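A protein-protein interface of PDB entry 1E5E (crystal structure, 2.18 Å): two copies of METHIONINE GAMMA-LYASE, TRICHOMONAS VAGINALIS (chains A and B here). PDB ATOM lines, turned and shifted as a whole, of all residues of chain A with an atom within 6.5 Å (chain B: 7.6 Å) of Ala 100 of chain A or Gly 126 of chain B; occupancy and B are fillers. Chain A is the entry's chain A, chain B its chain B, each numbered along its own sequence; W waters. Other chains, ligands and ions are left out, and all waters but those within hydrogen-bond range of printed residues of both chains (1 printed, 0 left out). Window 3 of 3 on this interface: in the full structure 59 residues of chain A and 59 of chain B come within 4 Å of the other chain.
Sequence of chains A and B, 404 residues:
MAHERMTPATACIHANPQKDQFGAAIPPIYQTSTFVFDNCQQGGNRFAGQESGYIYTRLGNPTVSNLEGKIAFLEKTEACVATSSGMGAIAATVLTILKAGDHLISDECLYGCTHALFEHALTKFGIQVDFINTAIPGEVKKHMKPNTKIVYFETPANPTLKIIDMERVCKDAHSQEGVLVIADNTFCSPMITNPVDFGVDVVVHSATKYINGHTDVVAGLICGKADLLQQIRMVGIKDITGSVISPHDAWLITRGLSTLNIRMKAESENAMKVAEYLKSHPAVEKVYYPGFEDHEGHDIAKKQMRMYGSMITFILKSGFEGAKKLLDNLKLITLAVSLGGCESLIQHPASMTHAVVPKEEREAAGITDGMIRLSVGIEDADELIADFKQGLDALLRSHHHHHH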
ATOM      1  N   LEU A  98     -12.915   5.784 -13.674  1.00  0.00           N
ATOM      2  CA  LEU A  98     -12.781   4.365 -13.971  1.00  0.00           C
ATOM      3  C   LEU A  98     -12.108   3.971 -15.265  1.00  0.00           C
ATOM      4  O   LEU A  98     -12.085   4.616 -16.314  1.00  0.00           O
ATOM      5  CB  LEU A  98     -14.192   3.757 -13.995  1.00  0.00           C
ATOM      6  CG  LEU A  98     -15.039   4.125 -12.765  1.00  0.00           C
ATOM      7  CD1 LEU A  98     -16.507   3.873 -13.066  1.00  0.00           C
ATOM      8  CD2 LEU A  98     -14.547   3.321 -11.572  1.00  0.00           C
ATOM      9  N   LYS A  99     -11.665   2.717 -15.263  1.00  0.00           N
ATOM     10  CA  LYS A  99     -11.042   2.041 -16.390  1.00  0.00           C
ATOM     11  C   LYS A  99     -11.441   0.568 -16.337  1.00  0.00           C
ATOM     12  O   LYS A  99     -11.893   0.111 -15.284  1.00  0.00           O
ATOM     13  CB  LYS A  99      -9.521   2.192 -16.323  1.00  0.00           C
ATOM     14  CG  LYS A  99      -8.911   1.540 -15.082  1.00  0.00           C
ATOM     15  CD  LYS A  99      -7.389   1.510 -15.209  1.00  0.00           C
ATOM     16  CE  LYS A  99      -6.672   1.498 -13.873  1.00  0.00           C
ATOM     17  NZ  LYS A  99      -7.203   0.547 -12.857  1.00  0.00           N
ATOM     18  N   ALA A 100     -11.450  -0.122 -17.455  1.00  0.00           N
ATOM     19  CA  ALA A 100     -11.760  -1.531 -17.540  1.00  0.00           C
ATOM     20  C   ALA A 100     -11.068  -2.280 -16.398  1.00  0.00           C
ATOM     21  O   ALA A 100      -9.914  -2.039 -16.078  1.00  0.00           O
ATOM     22  CB  ALA A 100     -11.414  -2.177 -18.891  1.00  0.00           C
ATOM     23  N   GLY A 101     -11.895  -3.046 -15.664  1.00  0.00           N
ATOM     24  CA  GLY A 101     -11.336  -3.746 -14.513  1.00  0.00           C
ATOM     25  C   GLY A 101     -11.666  -3.106 -13.180  1.00  0.00           C
ATOM     26  O   GLY A 101     -11.525  -3.811 -12.163  1.00  0.00           O
ATOM     27  N   ASP A 102     -12.011  -1.808 -13.152  1.00  0.00           N
ATOM     28  CA  ASP A 102     -12.356  -1.179 -11.882  1.00  0.00           C
ATOM     29  C   ASP A 102     -13.718  -1.673 -11.390  1.00  0.00           C
ATOM     30  O   ASP A 102     -14.451  -2.357 -12.085  1.00  0.00           O
ATOM     31  CB  ASP A 102     -12.401   0.342 -12.028  1.00  0.00           C
ATOM     32  CG  ASP A 102     -11.035   0.965 -12.160  1.00  0.00           C
ATOM     33  OD1 ASP A 102     -10.077   0.191 -11.909  1.00  0.00           O
ATOM     34  OD2 ASP A 102     -10.935   2.180 -12.476  1.00  0.00           O
ATOM     35  N   PHE A 125     -17.647  -2.018 -20.966  1.00  0.00           N
ATOM     36  CA  PHE A 125     -16.333  -1.413 -20.960  1.00  0.00           C
ATOM     37  C   PHE A 125     -15.463  -1.992 -19.866  1.00  0.00           C
ATOM     38  O   PHE A 125     -14.444  -1.443 -19.455  1.00  0.00           O
ATOM     39  CB  PHE A 125     -16.444   0.127 -20.797  1.00  0.00           C
ATOM     40  CG  PHE A 125     -17.042   0.746 -22.053  1.00  0.00           C
ATOM     41  CD1 PHE A 125     -16.699   0.368 -23.320  1.00  0.00           C
ATOM     42  CD2 PHE A 125     -17.935   1.812 -21.872  1.00  0.00           C
ATOM     43  CE1 PHE A 125     -17.252   0.981 -24.432  1.00  0.00           C
ATOM     44  CE2 PHE A 125     -18.501   2.422 -22.980  1.00  0.00           C
ATOM     45  CZ  PHE A 125     -18.181   1.988 -24.245  1.00  0.00           C
ATOM     46  N   GLY A 126     -15.887  -3.132 -19.314  1.00  0.00           N
ATOM     47  CA  GLY A 126     -15.103  -3.952 -18.416  1.00  0.00           C
ATOM     48  C   GLY A 126     -15.150  -3.449 -16.971  1.00  0.00           C
ATOM     49  O   GLY A 126     -14.198  -3.697 -16.219  1.00  0.00           O
ATOM     50  N   ILE A 127     -16.174  -2.665 -16.625  1.00  0.00           N
ATOM     51  CA  ILE A 127     -16.197  -2.133 -15.260  1.00  0.00           C
ATOM     52  C   ILE A 127     -17.085  -3.036 -14.423  1.00  0.00           C
ATOM     53  O   ILE A 127     -18.122  -3.404 -14.970  1.00  0.00           O
ATOM     54  CB  ILE A 127     -16.636  -0.651 -15.219  1.00  0.00           C
ATOM     55  CG1 ILE A 127     -15.476   0.207 -15.781  1.00  0.00           C
ATOM     56  CG2 ILE A 127     -16.930  -0.155 -13.807  1.00  0.00           C
ATOM     57  CD1 ILE A 127     -15.922   1.568 -16.269  1.00  0.00           C
ATOM     58  N   LYS B  99     -17.379  -2.073 -27.500  1.00  0.00           N
ATOM     59  CA  LYS B  99     -17.370  -2.629 -26.169  1.00  0.00           C
ATOM     60  C   LYS B  99     -15.960  -3.188 -25.970  1.00  0.00           C
ATOM     61  O   LYS B  99     -15.203  -3.339 -26.936  1.00  0.00           O
ATOM     62  CB  LYS B  99     -18.444  -3.687 -25.948  1.00  0.00           C
ATOM     63  CG  LYS B  99     -18.294  -4.831 -26.904  1.00  0.00           C
ATOM     64  CD  LYS B  99     -19.285  -5.954 -26.829  1.00  0.00           C
ATOM     65  CE  LYS B  99     -19.667  -6.616 -28.127  1.00  0.00           C
ATOM     66  NZ  LYS B  99     -18.812  -7.307 -29.115  1.00  0.00           N
ATOM     67  N   ALA B 100     -15.613  -3.538 -24.771  1.00  0.00           N
ATOM     68  CA  ALA B 100     -14.332  -4.070 -24.347  1.00  0.00           C
ATOM     69  C   ALA B 100     -14.053  -5.303 -25.195  1.00  0.00           C
ATOM     70  O   ALA B 100     -15.009  -6.060 -25.319  1.00  0.00           O
ATOM     71  CB  ALA B 100     -14.388  -4.443 -22.868  1.00  0.00           C
ATOM     72  N   GLY B 101     -12.914  -5.413 -25.845  1.00  0.00           N
ATOM     73  CA  GLY B 101     -12.683  -6.607 -26.666  1.00  0.00           C
ATOM     74  C   GLY B 101     -12.695  -6.310 -28.149  1.00  0.00           C
ATOM     75  O   GLY B 101     -12.157  -7.057 -28.974  1.00  0.00           O
ATOM     76  N   ASP B 102     -13.379  -5.264 -28.574  1.00  0.00           N
ATOM     77  CA  ASP B 102     -13.473  -4.847 -29.962  1.00  0.00           C
ATOM     78  C   ASP B 102     -12.171  -4.201 -30.423  1.00  0.00           C
ATOM     79  O   ASP B 102     -11.367  -3.761 -29.590  1.00  0.00           O
ATOM     80  CB  ASP B 102     -14.620  -3.836 -30.087  1.00  0.00           C
ATOM     81  CG  ASP B 102     -15.977  -4.511 -30.004  1.00  0.00           C
ATOM     82  OD1 ASP B 102     -16.054  -5.755 -29.979  1.00  0.00           O
ATOM     83  OD2 ASP B 102     -16.979  -3.771 -29.960  1.00  0.00           O
ATOM     84  N   HIS B 103     -12.041  -4.020 -31.718  1.00  0.00           N
ATOM     85  CA  HIS B 103     -10.874  -3.421 -32.335  1.00  0.00           C
ATOM     86  C   HIS B 103     -11.293  -2.282 -33.269  1.00  0.00           C
ATOM     87  O   HIS B 103     -12.258  -2.438 -34.015  1.00  0.00           O
ATOM     88  CB  HIS B 103     -10.172  -4.495 -33.181  1.00  0.00           C
ATOM     89  CG  HIS B 103      -8.925  -4.082 -33.889  1.00  0.00           C
ATOM     90  ND1 HIS B 103      -8.788  -4.297 -35.238  1.00  0.00           N
ATOM     91  CD2 HIS B 103      -7.779  -3.472 -33.475  1.00  0.00           C
ATOM     92  CE1 HIS B 103      -7.587  -3.877 -35.647  1.00  0.00           C
ATOM     93  NE2 HIS B 103      -6.979  -3.376 -34.588  1.00  0.00           N
ATOM     94  N   ALA B 121      -8.513   7.047 -24.199  1.00  0.00           N
ATOM     95  CA  ALA B 121      -9.784   6.667 -23.584  1.00  0.00           C
ATOM     96  C   ALA B 121     -10.245   5.306 -24.049  1.00  0.00           C
ATOM     97  O   ALA B 121     -10.555   4.475 -23.185  1.00  0.00           O
ATOM     98  CB  ALA B 121     -10.870   7.705 -23.804  1.00  0.00           C
ATOM     99  N   LEU B 122     -10.314   5.030 -25.342  1.00  0.00           N
ATOM    100  CA  LEU B 122     -10.844   3.739 -25.771  1.00  0.00           C
ATOM    101  C   LEU B 122      -9.968   2.599 -25.243  1.00  0.00           C
ATOM    102  O   LEU B 122     -10.510   1.576 -24.806  1.00  0.00           O
ATOM    103  CB  LEU B 122     -10.985   3.634 -27.288  1.00  0.00           C
ATOM    104  CG  LEU B 122     -11.761   4.721 -28.034  1.00  0.00           C
ATOM    105  CD1 LEU B 122     -11.930   4.385 -29.510  1.00  0.00           C
ATOM    106  CD2 LEU B 122     -13.158   4.900 -27.441  1.00  0.00           C
ATOM    107  N   THR B 123      -8.655   2.739 -25.252  1.00  0.00           N
ATOM    108  CA  THR B 123      -7.753   1.713 -24.791  1.00  0.00           C
ATOM    109  C   THR B 123      -7.944   1.468 -23.312  1.00  0.00           C
ATOM    110  O   THR B 123      -7.715   0.324 -22.938  1.00  0.00           O
ATOM    111  CB  THR B 123      -6.273   1.992 -25.083  1.00  0.00           C
ATOM    112  OG1 THR B 123      -5.864   3.218 -24.535  1.00  0.00           O
ATOM    113  CG2 THR B 123      -6.100   2.001 -26.616  1.00  0.00           C
ATOM    114  N   LYS B 124      -8.354   2.437 -22.465  1.00  0.00           N
ATOM    115  CA  LYS B 124      -8.625   2.063 -21.093  1.00  0.00           C
ATOM    116  C   LYS B 124      -9.981   1.384 -20.929  1.00  0.00           C
ATOM    117  O   LYS B 124     -10.279   0.877 -19.828  1.00  0.00           O
ATOM    118  CB  LYS B 124      -8.490   3.233 -20.088  1.00  0.00           C
ATOM    119  CG  LYS B 124      -9.561   4.296 -20.095  1.00  0.00           C
ATOM    120  CD  LYS B 124      -9.268   5.496 -19.180  1.00  0.00           C
ATOM    121  CE  LYS B 124     -10.630   6.217 -19.013  1.00  0.00           C
ATOM    122  NZ  LYS B 124     -10.750   6.831 -17.671  1.00  0.00           N
ATOM    123  N   PHE B 125     -10.835   1.389 -21.940  1.00  0.00           N
ATOM    124  CA  PHE B 125     -12.109   0.684 -21.849  1.00  0.00           C
ATOM    125  C   PHE B 125     -12.033  -0.676 -22.499  1.00  0.00           C
ATOM    126  O   PHE B 125     -13.057  -1.293 -22.797  1.00  0.00           O
ATOM    127  CB  PHE B 125     -13.270   1.547 -22.332  1.00  0.00           C
ATOM    128  CG  PHE B 125     -13.466   2.782 -21.506  1.00  0.00           C
ATOM    129  CD1 PHE B 125     -13.596   2.719 -20.136  1.00  0.00           C
ATOM    130  CD2 PHE B 125     -13.522   4.034 -22.102  1.00  0.00           C
ATOM    131  CE1 PHE B 125     -13.748   3.878 -19.385  1.00  0.00           C
ATOM    132  CE2 PHE B 125     -13.695   5.189 -21.372  1.00  0.00           C
ATOM    133  CZ  PHE B 125     -13.822   5.104 -19.998  1.00  0.00           C
ATOM    134  N   GLY B 126     -10.809  -1.179 -22.705  1.00  0.00           N
ATOM    135  CA  GLY B 126     -10.592  -2.502 -23.259  1.00  0.00           C
ATOM    136  C   GLY B 126     -10.698  -2.546 -24.761  1.00  0.00           C
ATOM    137  O   GLY B 126     -10.776  -3.646 -25.331  1.00  0.00           O
ATOM    138  N   ILE B 127     -10.742  -1.416 -25.462  1.00  0.00           N
ATOM    139  CA  ILE B 127     -10.844  -1.435 -26.934  1.00  0.00           C
ATOM    140  C   ILE B 127      -9.450  -1.401 -27.531  1.00  0.00           C
ATOM    141  O   ILE B 127      -8.577  -0.687 -27.034  1.00  0.00           O
ATOM    142  CB  ILE B 127     -11.692  -0.233 -27.406  1.00  0.00           C
ATOM    143  CG1 ILE B 127     -13.143  -0.482 -26.944  1.00  0.00           C
ATOM    144  CG2 ILE B 127     -11.622  -0.069 -28.911  1.00  0.00           C
ATOM    145  CD1 ILE B 127     -13.795   0.819 -26.497  1.00  0.00           C
ATOM    146  N   GLN B 128      -9.219  -2.187 -28.581  1.00  0.00           N
ATOM    147  CA  GLN B 128      -7.896  -2.186 -29.192  1.00  0.00           C
ATOM    148  C   GLN B 128      -7.892  -1.195 -30.357  1.00  0.00           C
ATOM    149  O   GLN B 128      -8.854  -1.173 -31.126  1.00  0.00           O
ATOM    150  CB  GLN B 128      -7.583  -3.574 -29.765  1.00  0.00           C
ATOM    151  CG  GLN B 128      -8.076  -4.715 -28.882  1.00  0.00           C
ATOM    152  CD  GLN B 128      -7.706  -6.065 -29.498  1.00  0.00           C
ATOM    153  OE1 GLN B 128      -8.486  -6.611 -30.296  1.00  0.00           O
ATOM    154  NE2 GLN B 128      -6.452  -6.453 -29.190  1.00  0.00           N
ATOM    155  N   VAL B 129      -6.805  -0.444 -30.496  1.00  0.00           N
ATOM    156  CA  VAL B 129      -6.738   0.511 -31.586  1.00  0.00           C
ATOM    157  C   VAL B 129      -5.434   0.442 -32.373  1.00  0.00           C
ATOM    158  O   VAL B 129      -4.356   0.400 -31.760  1.00  0.00           O
ATOM    159  CB  VAL B 129      -6.798   1.931 -30.945  1.00  0.00           C
ATOM    160  CG1 VAL B 129      -6.545   3.019 -31.957  1.00  0.00           C
ATOM    161  CG2 VAL B 129      -8.094   2.237 -30.210  1.00  0.00           C
ATOM    162  N   ASN B 147     -12.241  -9.327 -34.767  1.00  0.00           N
ATOM    163  CA  ASN B 147     -12.972  -8.446 -33.895  1.00  0.00           C
ATOM    164  C   ASN B 147     -12.974  -6.986 -34.334  1.00  0.00           C
ATOM    165  O   ASN B 147     -13.422  -6.109 -33.591  1.00  0.00           O
ATOM    166  CB  ASN B 147     -12.458  -8.516 -32.437  1.00  0.00           C
ATOM    167  CG  ASN B 147     -11.017  -8.075 -32.291  1.00  0.00           C
ATOM    168  OD1 ASN B 147     -10.194  -8.104 -33.218  1.00  0.00           O
ATOM    169  ND2 ASN B 147     -10.649  -7.622 -31.090  1.00  0.00           N
HETATM  170  O   HOH W   1      -9.138   5.785 -15.536  1.00  0.00           O
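The backbone carbonyl oxygen of Lys 124 of chain B lies within hydrogen-bond range of the backbone NH of Ala 100 of chain A (2.8 Å). The backbone carbonyl oxygen of Leu 98 of chain A is in hydrogen-bond range of the side-chain amino group of Lys 124 of chain B (2.9 Å).
Of the 8 printed residues of chain A, 4 touch a printed residue of chain B. Printed residues of chain A that touch a printed residue of chain B: Leu 98, Lys 99, Ala 100 and Phe 125. Hydrophobic or aromatic side chains of chain A that line the printed part of chain B: Ala 100 and Phe 125. Of the 15 printed residues of chain B, 3 touch a printed residue of chain A. Printed residues of chain B that touch a printed residue of chain A: Lys 124, Phe 125 and Gly 126. Among the printed residues, 7 pairs touch across the chains. Among the printed residues, no Asp or Glu carboxylate lies within 4 Å of a Lys or Arg side-chain nitrogen of the other chain.
The side-chain amino group (NZ) of Lys 99 of chain A is in salt-bridge range of the side-chain carboxylate (OD1) of Asp 102 of chain A, 3.0 Å away. The backbone carbonyl oxygen (O) of Gly 126 of chain B lies within hydrogen-bond range of the backbone NH (N) of Gly 101 of chain B (2.8 Å).
Water W1 bridges NZ of Lys 124 of chain B and O of Leu 98 of chain A.
Leu 98 of chain A touches Phe 125 of chain B. Lys 99 of chain A touches Lys 124 of chain B. Phe 125 of chain B touches Ala 100 of chain A (C to CB, 3.96 Å). Gly 126 of chain B touches Ala 100 of chain A. Phe 125 of chain A touches Phe 125 of chain B (O to O, 3.6 Å).
Ala 100 of chain A touches Phe 125 of chain B, but with the chains exchanged Phe 125 of chain A does not touch Ala 100 of chain B (4.02 Å). Ala 100 of chain A touches Gly 126 of chain B, but with the chains exchanged Gly 126 of chain A does not touch Ala 100 of chain B (4.1 Å). Phe 125 of chain B touches its own counterpart, Phe 125 of chain A.
Printed residues of chain B within 4 Å of Ala 100 of chain A: Lys 124 (2.8 Å), Phe 125 (3.96 Å) and Gly 126 (3.99 Å). Of the printed residues of chain A, Gly 126 of chain B touches Ala 100. Of the printed residues of chain A, Lys 124 of chain B touches Leu 98 (2.9 Å), Lys 99 (3.7 Å) and Ala 100 (2.8 Å). Printed residues of chain B within 4 Å of Lys 99 of chain A: Lys 124 (3.7 Å). The nearest printed residue of chain B that does not touch Ala 100 of chain A is Ala 100 of chain B (5.5 Å). The nearest printed residue of chain B that does not touch Lys 99 of chain A is Phe 125 of chain B (4.4 Å).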
